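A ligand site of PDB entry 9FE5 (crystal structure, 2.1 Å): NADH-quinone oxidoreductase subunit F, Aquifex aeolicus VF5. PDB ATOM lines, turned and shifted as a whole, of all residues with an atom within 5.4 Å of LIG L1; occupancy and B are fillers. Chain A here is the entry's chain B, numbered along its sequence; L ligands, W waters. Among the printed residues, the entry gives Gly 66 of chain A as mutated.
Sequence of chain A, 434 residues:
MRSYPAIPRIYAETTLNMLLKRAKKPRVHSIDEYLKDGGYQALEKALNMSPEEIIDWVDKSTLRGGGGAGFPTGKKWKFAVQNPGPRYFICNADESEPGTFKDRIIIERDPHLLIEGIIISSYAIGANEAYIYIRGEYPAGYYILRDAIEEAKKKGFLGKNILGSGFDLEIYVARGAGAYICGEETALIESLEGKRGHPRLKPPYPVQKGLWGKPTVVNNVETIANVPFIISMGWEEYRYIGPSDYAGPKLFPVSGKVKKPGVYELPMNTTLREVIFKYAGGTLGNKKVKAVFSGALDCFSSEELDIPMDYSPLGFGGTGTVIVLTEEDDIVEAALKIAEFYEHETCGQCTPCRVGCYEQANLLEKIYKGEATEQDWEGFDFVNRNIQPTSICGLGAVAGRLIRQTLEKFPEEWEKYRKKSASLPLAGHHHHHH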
ATOM      1  N   GLY A  66      12.754  14.098   3.152  1.00  0.00           N
ATOM      2  CA  GLY A  66      14.198  14.241   3.077  1.00  0.00           C
ATOM      3  C   GLY A  66      14.653  15.640   3.453  1.00  0.00           C
ATOM      4  O   GLY A  66      15.815  15.993   3.273  1.00  0.00           O
ATOM      5  N   GLY A  67      13.709  16.438   3.991  1.00  0.00           N
ATOM      6  CA  GLY A  67      13.988  17.802   4.407  1.00  0.00           C
ATOM      7  C   GLY A  67      14.539  17.882   5.823  1.00  0.00           C
ATOM      8  O   GLY A  67      14.873  18.965   6.290  1.00  0.00           O
ATOM      9  N   GLY A  68      14.578  16.749   6.542  1.00  0.00           N
ATOM     10  CA  GLY A  68      15.303  16.679   7.808  1.00  0.00           C
ATOM     11  C   GLY A  68      14.517  16.005   8.926  1.00  0.00           C
ATOM     12  O   GLY A  68      15.112  15.397   9.814  1.00  0.00           O
ATOM     13  N   ALA A  69      13.182  16.095   8.898  1.00  0.00           N
ATOM     14  CA  ALA A  69      12.364  15.552   9.984  1.00  0.00           C
ATOM     15  C   ALA A  69      11.898  14.125   9.705  1.00  0.00           C
ATOM     16  O   ALA A  69      11.405  13.455  10.607  1.00  0.00           O
ATOM     17  CB  ALA A  69      11.194  16.472  10.237  1.00  0.00           C
ATOM     18  N   PHE A  71       9.302  12.933   8.164  1.00  0.00           N
ATOM     19  CA  PHE A  71       7.884  12.692   8.384  1.00  0.00           C
ATOM     20  C   PHE A  71       7.314  11.868   7.231  1.00  0.00           C
ATOM     21  O   PHE A  71       7.615  12.148   6.069  1.00  0.00           O
ATOM     22  CB  PHE A  71       7.104  14.000   8.570  1.00  0.00           C
ATOM     23  CG  PHE A  71       5.683  13.812   9.056  1.00  0.00           C
ATOM     24  CD1 PHE A  71       5.393  13.732  10.408  1.00  0.00           C
ATOM     25  CD2 PHE A  71       4.622  13.694   8.157  1.00  0.00           C
ATOM     26  CE1 PHE A  71       4.086  13.542  10.861  1.00  0.00           C
ATOM     27  CE2 PHE A  71       3.321  13.519   8.598  1.00  0.00           C
ATOM     28  CZ  PHE A  71       3.053  13.444   9.951  1.00  0.00           C
ATOM     29  N   LYS A  76       1.210  12.776   5.458  1.00  0.00           N
ATOM     30  CA  LYS A  76       1.118  14.218   5.295  1.00  0.00           C
ATOM     31  C   LYS A  76       0.047  14.561   4.261  1.00  0.00           C
ATOM     32  O   LYS A  76      -0.816  15.409   4.502  1.00  0.00           O
ATOM     33  CB  LYS A  76       2.469  14.813   4.888  1.00  0.00           C
ATOM     34  CG  LYS A  76       2.540  16.328   5.014  1.00  0.00           C
ATOM     35  CD  LYS A  76       3.826  16.990   4.506  1.00  0.00           C
ATOM     36  CE  LYS A  76       5.072  16.647   5.258  1.00  0.00           C
ATOM     37  NZ  LYS A  76       6.167  17.527   4.845  1.00  0.00           N
ATOM     38  N   PHE A  79      -3.512  13.998   5.388  1.00  0.00           N
ATOM     39  CA  PHE A  79      -3.975  15.069   6.244  1.00  0.00           C
ATOM     40  C   PHE A  79      -4.497  16.232   5.391  1.00  0.00           C
ATOM     41  O   PHE A  79      -5.569  16.768   5.666  1.00  0.00           O
ATOM     42  CB  PHE A  79      -2.859  15.457   7.221  1.00  0.00           C
ATOM     43  CG  PHE A  79      -2.646  14.505   8.400  1.00  0.00           C
ATOM     44  CD1 PHE A  79      -3.706  13.817   8.987  1.00  0.00           C
ATOM     45  CD2 PHE A  79      -1.364  14.328   8.937  1.00  0.00           C
ATOM     46  CE1 PHE A  79      -3.491  12.986  10.084  1.00  0.00           C
ATOM     47  CE2 PHE A  79      -1.171  13.486  10.026  1.00  0.00           C
ATOM     48  CZ  PHE A  79      -2.231  12.823  10.594  1.00  0.00           C
ATOM     49  N   GLU A  95      17.326  24.640   0.741  1.00  0.00           N
ATOM     50  CA  GLU A  95      18.586  24.007   1.121  1.00  0.00           C
ATOM     51  C   GLU A  95      19.673  25.001   1.514  1.00  0.00           C
ATOM     52  O   GLU A  95      20.489  25.397   0.685  1.00  0.00           O
ATOM     53  CB  GLU A  95      19.078  23.148  -0.050  1.00  0.00           C
ATOM     54  CG  GLU A  95      20.331  22.348   0.293  1.00  0.00           C
ATOM     55  CD  GLU A  95      20.619  21.250  -0.708  1.00  0.00           C
ATOM     56  OE1 GLU A  95      21.020  21.600  -1.847  1.00  0.00           O
ATOM     57  OE2 GLU A  95      20.448  20.070  -0.356  1.00  0.00           O
ATOM     58  N   SER A  96      19.732  25.348   2.814  1.00  0.00           N
ATOM     59  CA  SER A  96      20.743  26.255   3.316  1.00  0.00           C
ATOM     60  C   SER A  96      21.437  25.788   4.607  1.00  0.00           C
ATOM     61  O   SER A  96      22.241  26.548   5.155  1.00  0.00           O
ATOM     62  CB  SER A  96      20.157  27.634   3.487  1.00  0.00           C
ATOM     63  OG  SER A  96      19.840  28.201   2.224  1.00  0.00           O
ATOM     64  N   GLU A  97      21.172  24.565   5.082  1.00  0.00           N
ATOM     65  CA  GLU A  97      21.834  24.067   6.279  1.00  0.00           C
ATOM     66  C   GLU A  97      23.285  23.725   5.933  1.00  0.00           C
ATOM     67  O   GLU A  97      23.549  23.029   4.957  1.00  0.00           O
ATOM     68  CB  GLU A  97      21.141  22.847   6.892  1.00  0.00           C
ATOM     69  CG  GLU A  97      21.742  22.413   8.234  1.00  0.00           C
ATOM     70  CD  GLU A  97      21.012  21.314   8.977  1.00  0.00           C
ATOM     71  OE1 GLU A  97      19.935  20.860   8.532  1.00  0.00           O
ATOM     72  OE2 GLU A  97      21.527  20.904  10.043  1.00  0.00           O
ATOM     73  N   THR A 100      24.942  20.804   3.547  1.00  0.00           N
ATOM     74  CA  THR A 100      23.845  20.168   2.807  1.00  0.00           C
ATOM     75  C   THR A 100      23.751  20.752   1.398  1.00  0.00           C
ATOM     76  O   THR A 100      23.436  21.927   1.233  1.00  0.00           O
ATOM     77  CB  THR A 100      22.538  20.332   3.584  1.00  0.00           C
ATOM     78  OG1 THR A 100      22.846  19.990   4.937  1.00  0.00           O
ATOM     79  CG2 THR A 100      21.430  19.452   3.034  1.00  0.00           C
ATOM     80  N   LYS A 102      22.632  18.293  -1.281  1.00  0.00           N
ATOM     81  CA  LYS A 102      22.056  17.151  -1.969  1.00  0.00           C
ATOM     82  C   LYS A 102      20.969  17.592  -2.966  1.00  0.00           C
ATOM     83  O   LYS A 102      20.881  17.044  -4.060  1.00  0.00           O
ATOM     84  CB  LYS A 102      21.523  16.155  -0.931  1.00  0.00           C
ATOM     85  CG  LYS A 102      20.460  16.694   0.023  1.00  0.00           C
ATOM     86  CD  LYS A 102      19.897  15.661   0.995  1.00  0.00           C
ATOM     87  CE  LYS A 102      18.778  16.219   1.823  1.00  0.00           C
ATOM     88  NZ  LYS A 102      17.527  16.340   1.066  1.00  0.00           N
ATOM     89  N   ASP A 103      20.130  18.553  -2.593  1.00  0.00           N
ATOM     90  CA  ASP A 103      18.964  18.882  -3.412  1.00  0.00           C
ATOM     91  C   ASP A 103      19.371  19.567  -4.710  1.00  0.00           C
ATOM     92  O   ASP A 103      18.734  19.359  -5.744  1.00  0.00           O
ATOM     93  CB  ASP A 103      17.978  19.744  -2.649  1.00  0.00           C
ATOM     94  CG  ASP A 103      17.374  19.121  -1.403  1.00  0.00           C
ATOM     95  OD1 ASP A 103      17.425  17.870  -1.282  1.00  0.00           O
ATOM     96  OD2 ASP A 103      16.892  19.890  -0.544  1.00  0.00           O
ATOM     97  N   TYR A 180      18.127  31.714   5.904  1.00  0.00           N
ATOM     98  CA  TYR A 180      18.048  30.285   6.158  1.00  0.00           C
ATOM     99  C   TYR A 180      16.679  29.893   6.710  1.00  0.00           C
ATOM    100  O   TYR A 180      16.202  28.791   6.480  1.00  0.00           O
ATOM    101  CB  TYR A 180      19.154  29.880   7.143  1.00  0.00           C
ATOM    102  CG  TYR A 180      18.993  28.549   7.859  1.00  0.00           C
ATOM    103  CD1 TYR A 180      19.225  27.345   7.215  1.00  0.00           C
ATOM    104  CD2 TYR A 180      18.664  28.502   9.219  1.00  0.00           C
ATOM    105  CE1 TYR A 180      19.111  26.132   7.870  1.00  0.00           C
ATOM    106  CE2 TYR A 180      18.557  27.300   9.892  1.00  0.00           C
ATOM    107  CZ  TYR A 180      18.769  26.103   9.213  1.00  0.00           C
ATOM    108  OH  TYR A 180      18.657  24.925   9.881  1.00  0.00           O
ATOM    109  N   GLU A 184      12.310  26.894   6.762  1.00  0.00           N
ATOM    110  CA  GLU A 184      11.248  26.480   7.671  1.00  0.00           C
ATOM    111  C   GLU A 184       9.920  26.692   6.946  1.00  0.00           C
ATOM    112  O   GLU A 184       9.684  27.771   6.407  1.00  0.00           O
ATOM    113  CB  GLU A 184      11.321  27.248   8.987  1.00  0.00           C
ATOM    114  CG  GLU A 184      10.569  26.585  10.139  1.00  0.00           C
ATOM    115  CD  GLU A 184       9.065  26.793  10.186  1.00  0.00           C
ATOM    116  OE1 GLU A 184       8.550  27.734   9.546  1.00  0.00           O
ATOM    117  OE2 GLU A 184       8.403  25.999  10.903  1.00  0.00           O
ATOM    118  N   GLU A 185       9.068  25.668   6.932  1.00  0.00           N
ATOM    119  CA  GLU A 185       7.939  25.611   6.012  1.00  0.00           C
ATOM    120  C   GLU A 185       6.984  26.792   6.183  1.00  0.00           C
ATOM    121  O   GLU A 185       6.490  27.304   5.180  1.00  0.00           O
ATOM    122  CB  GLU A 185       7.224  24.265   6.106  1.00  0.00           C
ATOM    123  CG  GLU A 185       6.517  24.039   7.435  1.00  0.00           C
ATOM    124  CD  GLU A 185       5.884  22.670   7.558  1.00  0.00           C
ATOM    125  OE1 GLU A 185       5.840  21.940   6.537  1.00  0.00           O
ATOM    126  OE2 GLU A 185       5.430  22.357   8.685  1.00  0.00           O
ATOM    127  N   LYS A 202       2.960  26.436  15.124  1.00  0.00           N
ATOM    128  CA  LYS A 202       2.390  25.170  14.677  1.00  0.00           C
ATOM    129  C   LYS A 202       2.029  24.326  15.903  1.00  0.00           C
ATOM    130  O   LYS A 202       2.826  24.262  16.842  1.00  0.00           O
ATOM    131  CB  LYS A 202       3.383  24.362  13.848  1.00  0.00           C
ATOM    132  CG  LYS A 202       3.865  25.013  12.562  1.00  0.00           C
ATOM    133  CD  LYS A 202       5.293  24.625  12.159  1.00  0.00           C
ATOM    134  CE  LYS A 202       5.499  23.191  11.807  1.00  0.00           C
ATOM    135  NZ  LYS A 202       6.781  22.997  11.101  1.00  0.00           N
ATOM    136  N   TYR A 205      -0.613  22.981  11.298  1.00  0.00           N
ATOM    137  CA  TYR A 205       0.371  22.601  10.309  1.00  0.00           C
ATOM    138  C   TYR A 205      -0.104  23.111   8.939  1.00  0.00           C
ATOM    139  O   TYR A 205      -1.293  23.346   8.742  1.00  0.00           O
ATOM    140  CB  TYR A 205       0.614  21.082  10.337  1.00  0.00           C
ATOM    141  CG  TYR A 205       1.313  20.611  11.607  1.00  0.00           C
ATOM    142  CD1 TYR A 205       2.678  20.735  11.766  1.00  0.00           C
ATOM    143  CD2 TYR A 205       0.584  20.054  12.667  1.00  0.00           C
ATOM    144  CE1 TYR A 205       3.312  20.331  12.936  1.00  0.00           C
ATOM    145  CE2 TYR A 205       1.206  19.644  13.839  1.00  0.00           C
ATOM    146  CZ  TYR A 205       2.572  19.780  13.963  1.00  0.00           C
ATOM    147  OH  TYR A 205       3.204  19.381  15.103  1.00  0.00           O
ATOM    148  N   PRO A 206       0.805  23.309   7.959  1.00  0.00           N
ATOM    149  CA  PRO A 206       0.409  23.814   6.642  1.00  0.00           C
ATOM    150  C   PRO A 206      -0.733  23.049   5.984  1.00  0.00           C
ATOM    151  O   PRO A 206      -1.553  23.653   5.295  1.00  0.00           O
ATOM    152  CB  PRO A 206       1.720  23.697   5.842  1.00  0.00           C
ATOM    153  CG  PRO A 206       2.784  23.900   6.893  1.00  0.00           C
ATOM    154  CD  PRO A 206       2.263  23.096   8.076  1.00  0.00           C
ATOM    155  N   VAL A 207      -0.799  21.730   6.218  1.00  0.00           N
ATOM    156  CA  VAL A 207      -1.791  20.879   5.573  1.00  0.00           C
ATOM    157  C   VAL A 207      -3.192  21.276   6.037  1.00  0.00           C
ATOM    158  O   VAL A 207      -4.162  20.952   5.364  1.00  0.00           O
ATOM    159  CB  VAL A 207      -1.545  19.374   5.782  1.00  0.00           C
ATOM    160  CG1 VAL A 207      -0.274  18.909   5.070  1.00  0.00           C
ATOM    161  CG2 VAL A 207      -1.529  18.973   7.241  1.00  0.00           C
ATOM    162  N   VAL A 218       3.931  21.077   2.009  1.00  0.00           N
ATOM    163  CA  VAL A 218       5.317  21.423   1.740  1.00  0.00           C
ATOM    164  C   VAL A 218       6.138  20.137   1.799  1.00  0.00           C
ATOM    165  O   VAL A 218       6.075  19.422   2.788  1.00  0.00           O
ATOM    166  CB  VAL A 218       5.847  22.455   2.750  1.00  0.00           C
ATOM    167  CG1 VAL A 218       7.263  22.917   2.406  1.00  0.00           C
ATOM    168  CG2 VAL A 218       4.907  23.648   2.874  1.00  0.00           C
ATOM    169  N   ASN A 220      10.222  18.563   0.601  1.00  0.00           N
ATOM    170  CA  ASN A 220      11.593  18.792   0.165  1.00  0.00           C
ATOM    171  C   ASN A 220      11.808  18.219  -1.235  1.00  0.00           C
ATOM    172  O   ASN A 220      11.142  17.268  -1.637  1.00  0.00           O
ATOM    173  CB  ASN A 220      12.523  18.210   1.225  1.00  0.00           C
ATOM    174  CG  ASN A 220      13.978  18.263   0.838  1.00  0.00           C
ATOM    175  OD1 ASN A 220      14.625  19.311   0.956  1.00  0.00           O
ATOM    176  ND2 ASN A 220      14.514  17.129   0.428  1.00  0.00           N
ATOM    177  N   LEU A 297      23.156  20.394  13.292  1.00  0.00           N
ATOM    178  CA  LEU A 297      22.135  19.798  14.132  1.00  0.00           C
ATOM    179  C   LEU A 297      22.752  18.944  15.244  1.00  0.00           C
ATOM    180  O   LEU A 297      22.456  19.166  16.422  1.00  0.00           O
ATOM    181  CB  LEU A 297      21.193  18.977  13.253  1.00  0.00           C
ATOM    182  CG  LEU A 297      19.947  18.419  13.941  1.00  0.00           C
ATOM    183  CD1 LEU A 297      19.071  19.548  14.471  1.00  0.00           C
ATOM    184  CD2 LEU A 297      19.157  17.542  12.975  1.00  0.00           C
ATOM    185  N   GLY A 318      17.997  12.976  10.014  1.00  0.00           N
ATOM    186  CA  GLY A 318      18.227  14.295   9.458  1.00  0.00           C
ATOM    187  C   GLY A 318      18.200  14.262   7.930  1.00  0.00           C
ATOM    188  O   GLY A 318      17.427  13.504   7.347  1.00  0.00           O
ATOM    189  N   THR A 319      19.069  15.079   7.314  1.00  0.00           N
ATOM    190  CA  THR A 319      19.204  15.149   5.869  1.00  0.00           C
ATOM    191  C   THR A 319      20.333  14.233   5.389  1.00  0.00           C
ATOM    192  O   THR A 319      20.673  14.280   4.211  1.00  0.00           O
ATOM    193  CB  THR A 319      19.431  16.601   5.440  1.00  0.00           C
ATOM    194  OG1 THR A 319      20.568  17.069   6.165  1.00  0.00           O
ATOM    195  CG2 THR A 319      18.207  17.455   5.699  1.00  0.00           C
ATOM    196  N   GLY A 394      11.935  25.194  14.952  1.00  0.00           N
ATOM    197  CA  GLY A 394      13.000  24.247  15.281  1.00  0.00           C
ATOM    198  C   GLY A 394      14.372  24.904  15.431  1.00  0.00           C
ATOM    199  O   GLY A 394      15.238  24.341  16.094  1.00  0.00           O
HETATM  200  P1  LIG L   1       8.484  18.819  12.097  1.00  0.00           P
HETATM  201  O1  LIG L   1       8.732  17.537  12.771  1.00  0.00           O
HETATM  202  O2  LIG L   1       7.712  19.817  12.925  1.00  0.00           O
HETATM  203  O3  LIG L   1       7.616  18.627  10.771  1.00  0.00           O
HETATM  204  C1  LIG L   1       8.094  17.879   9.638  1.00  0.00           C
HETATM  205  C2  LIG L   1       7.046  17.909   8.560  1.00  0.00           C
HETATM  206  O4  LIG L   1       5.934  17.065   8.942  1.00  0.00           O
HETATM  207  C3  LIG L   1       6.450  19.287   8.282  1.00  0.00           C
HETATM  208  O5  LIG L   1       6.099  19.419   6.920  1.00  0.00           O
HETATM  209  C4  LIG L   1       5.210  19.308   9.181  1.00  0.00           C
HETATM  210  O6  LIG L   1       4.202  20.174   8.682  1.00  0.00           O
HETATM  211  C5  LIG L   1       4.753  17.852   9.080  1.00  0.00           C
HETATM  212  N1  LIG L   1       4.011  17.389  10.243  1.00  0.00           N
HETATM  213  C6  LIG L   1       4.515  16.973  11.454  1.00  0.00           C
HETATM  214  N2  LIG L   1       3.598  16.606  12.323  1.00  0.00           N
HETATM  215  C7  LIG L   1       2.403  16.795  11.635  1.00  0.00           C
HETATM  216  C8  LIG L   1       1.056  16.569  11.983  1.00  0.00           C
HETATM  217  N3  LIG L   1       0.673  16.093  13.171  1.00  0.00           N
HETATM  218  N4  LIG L   1       0.111  16.864  11.071  1.00  0.00           N
HETATM  219  C9  LIG L   1       0.496  17.353   9.884  1.00  0.00           C
HETATM  220  N5  LIG L   1       1.728  17.596   9.430  1.00  0.00           N
HETATM  221  C10 LIG L   1       2.646  17.281  10.354  1.00  0.00           C
HETATM  222  O7  LIG L   1       9.862  19.477  11.631  1.00  0.00           O
HETATM  223  P2  LIG L   1      10.351  20.894  11.076  1.00  0.00           P
HETATM  224  O8  LIG L   1      10.180  21.882  12.233  1.00  0.00           O
HETATM  225  O9  LIG L   1       9.603  21.297   9.864  1.00  0.00           O
HETATM  226  O10 LIG L   1      11.941  20.694  10.730  1.00  0.00           O
HETATM  227  C11 LIG L   1      13.126  20.562  11.562  1.00  0.00           C
HETATM  228  C12 LIG L   1      14.199  19.878  10.750  1.00  0.00           C
HETATM  229  O11 LIG L   1      14.654  20.717   9.671  1.00  0.00           O
HETATM  230  C13 LIG L   1      15.475  19.453  11.494  1.00  0.00           C
HETATM  231  O12 LIG L   1      15.412  18.059  11.749  1.00  0.00           O
HETATM  232  C14 LIG L   1      16.618  19.781  10.510  1.00  0.00           C
HETATM  233  O13 LIG L   1      17.458  18.668  10.231  1.00  0.00           O
HETATM  234  C15 LIG L   1      15.863  20.146   9.225  1.00  0.00           C
HETATM  235  N6  LIG L   1      16.557  21.079   8.326  1.00  0.00           N
HETATM  236  C16 LIG L   1      16.959  20.704   6.938  1.00  0.00           C
HETATM  237  C17 LIG L   1      17.492  21.582   6.058  1.00  0.00           C
HETATM  238  C18 LIG L   1      17.847  21.233   4.630  1.00  0.00           C
HETATM  239  O14 LIG L   1      18.643  21.935   3.979  1.00  0.00           O
HETATM  240  N7  LIG L   1      17.261  20.189   4.070  1.00  0.00           N
HETATM  241  C19 LIG L   1      17.726  22.970   6.500  1.00  0.00           C
HETATM  242  C20 LIG L   1      17.463  23.204   7.942  1.00  0.00           C
HETATM  243  C21 LIG L   1      16.898  22.326   8.754  1.00  0.00           C
HETATM  244  C1  LG2 L   2      13.687  23.452   7.820  1.00  0.00           C
HETATM  245  N1  LG2 L   2      13.226  22.489   6.869  1.00  0.00           N
HETATM  246  C2  LG2 L   2      13.776  22.489   5.593  1.00  0.00           C
HETATM  247  N2  LG2 L   2      13.301  21.572   4.680  1.00  0.00           N
HETATM  248  C3  LG2 L   2      13.694  21.576   3.365  1.00  0.00           C
HETATM  249  O1  LG2 L   2      13.149  20.866   2.522  1.00  0.00           O
HETATM  250  N3  LG2 L   2      14.691  22.448   3.033  1.00  0.00           N
HETATM  251  C4  LG2 L   2      15.261  23.410   3.860  1.00  0.00           C
HETATM  252  O2  LG2 L   2      16.132  24.157   3.416  1.00  0.00           O
HETATM  253  C5  LG2 L   2      14.733  23.397   5.201  1.00  0.00           C
HETATM  254  N4  LG2 L   2      15.146  24.347   6.092  1.00  0.00           N
HETATM  255  C6  LG2 L   2      14.648  24.387   7.395  1.00  0.00           C
HETATM  256  C7  LG2 L   2      15.100  25.369   8.279  1.00  0.00           C
HETATM  257  C8  LG2 L   2      14.622  25.419   9.590  1.00  0.00           C
HETATM  258  C9  LG2 L   2      15.146  26.478  10.527  1.00  0.00           C
HETATM  259  C10 LG2 L   2      13.670  24.469  10.016  1.00  0.00           C
HETATM  260  C11 LG2 L   2      13.163  24.469  11.439  1.00  0.00           C
HETATM  261  C12 LG2 L   2      13.210  23.502   9.132  1.00  0.00           C
HETATM  262  C13 LG2 L   2      12.160  21.550   7.217  1.00  0.00           C
HETATM  263  C14 LG2 L   2      10.813  22.091   6.755  1.00  0.00           C
HETATM  264  O3  LG2 L   2      10.298  22.965   7.758  1.00  0.00           O
HETATM  265  C15 LG2 L   2       9.844  20.934   6.483  1.00  0.00           C
HETATM  266  O4  LG2 L   2       9.889  19.991   7.552  1.00  0.00           O
HETATM  267  C16 LG2 L   2      10.093  20.200   5.163  1.00  0.00           C
HETATM  268  O5  LG2 L   2      10.301  21.108   4.069  1.00  0.00           O
HETATM  269  C17 LG2 L   2       8.961  19.250   4.843  1.00  0.00           C
HETATM  270  O6  LG2 L   2       9.302  18.458   3.686  1.00  0.00           O
HETATM  271  P1  LG2 L   2       9.604  16.883   3.882  1.00  0.00           P
HETATM  272  O7  LG2 L   2       8.507  16.302   4.738  1.00  0.00           O
HETATM  273  O8  LG2 L   2      10.974  16.729   4.530  1.00  0.00           O
HETATM  274  O9  LG2 L   2       9.578  16.388   2.448  1.00  0.00           O
HETATM  275  O   HOH W   1      18.551  19.691   1.554  1.00  0.00           O
HETATM  276  O   HOH W   2       9.848  24.375  12.836  1.00  0.00           O
HETATM  277  O   HOH W   3       2.114  19.626   7.325  1.00  0.00           O
HETATM  278  O   HOH W   4      -2.331  16.790  11.774  1.00  0.00           O
HETATM  279  O   HOH W   5      20.292  19.666   6.001  1.00  0.00           O
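A nitrogen (N2) of LG2 L2 sits at hydrogen-bond distance from the backbone carbonyl oxygen of Gly 67 (3.4 Å). The backbone carbonyl oxygen (O) of Gly 68 sits at hydrogen-bond distance from an oxygen (O12) of LIG L1 (3.3 Å). N of Gly 66 sits at hydrogen-bond distance from O8 of LG2 L2, at 3.5 Å. An oxygen (O2) of LG2 L2 lies within hydrogen-bond range of the backbone NH (N) of Glu 95 (3.0 Å). The backbone NH (N) of Glu 185 sits at hydrogen-bond distance from an oxygen (O3) of LG2 L2, at 3.1 Å. The side-chain amino group of Lys 76 lies within hydrogen-bond range of an oxygen (O5) of LIG L1. N of Gly 67 is in hydrogen-bond range of O8 of LG2 L2. An oxygen (O1) of LG2 L2 lies close to the side-chain amide oxygen (OD1) of Asn 220 (2.7 Å). O7 of LG2 L2 is in salt-bridge range of NZ of Lys 76 (2.6 Å). N7 of LIG L1 sits close to O of Gly 67 (3.5 Å). The side-chain amino group (NZ) of Lys 202 lies within salt-bridge range of an oxygen (O9) of LIG L1, at 3.5 Å. The backbone NH of Asn 220 is in hydrogen-bond range of an oxygen (O9) of LG2 L2 (2.9 Å). An oxygen (O6) of LIG L1 sits at hydrogen-bond distance from the side-chain carboxylate of Glu 185, at 2.5 Å. The side-chain carboxylate of Glu 97 sits close to a nitrogen (N6) of LIG L1 (3.4 Å).
O9 of LIG L1 is in hydrogen-bond range of O4 of LG2 L2, 2.7 Å away.
The side-chain carboxylate of Glu 95 sits at hydrogen-bond distance from the backbone NH of Asp 103 (2.7 Å). The side-chain carboxylate of Glu 95 is in hydrogen-bond range of the backbone NH of Lys 102 (3.0 Å). O of Glu 97 sits at hydrogen-bond distance from OG1 of Thr 100, 3.1 Å away. NZ of Lys 76 sits at hydrogen-bond distance from O of Val 218 (2.8 Å). OE2 of Glu 185 lies within salt-bridge range of NZ of Lys 202 (2.8 Å). NZ of Lys 202 lies within salt-bridge range of OE2 of Glu 184, at 3.4 Å.
Residues that only touch LIG L1: Tyr 180, Phe 71, Thr 319, Leu 297, Ala 69, Tyr 205, Glu 95, Pro 206, Phe 79, Val 207, Ser 96 and Thr 100. Hydrophobic or aromatic side chains that line LIG L1: Ala 69, Phe 71, Phe 79, Tyr 180, Tyr 205, Pro 206, Val 207 and Leu 297. Of the 26 residues printed, 18 come within 4 Å of LIG L1. The nearest printed residue that does not touch LIG L1 is Val 218 (4.1 Å).
Water W2 lies within hydrogen-bond range of O8 of LIG L1 (2.6 Å), OE2 of Glu 184 (2.9 Å) and N of Gly 394 (3.1 Å). Water W1 lies within hydrogen-bond range of the side-chain carboxylate of Asp 103, the side-chain carboxylate of Glu 95 and a nitrogen (N7) of LIG L1. Water W5 lies within hydrogen-bond range of OG1 of Thr 319, OG1 of Thr 100, OE1 of Glu 97 and O14 of LIG L1.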
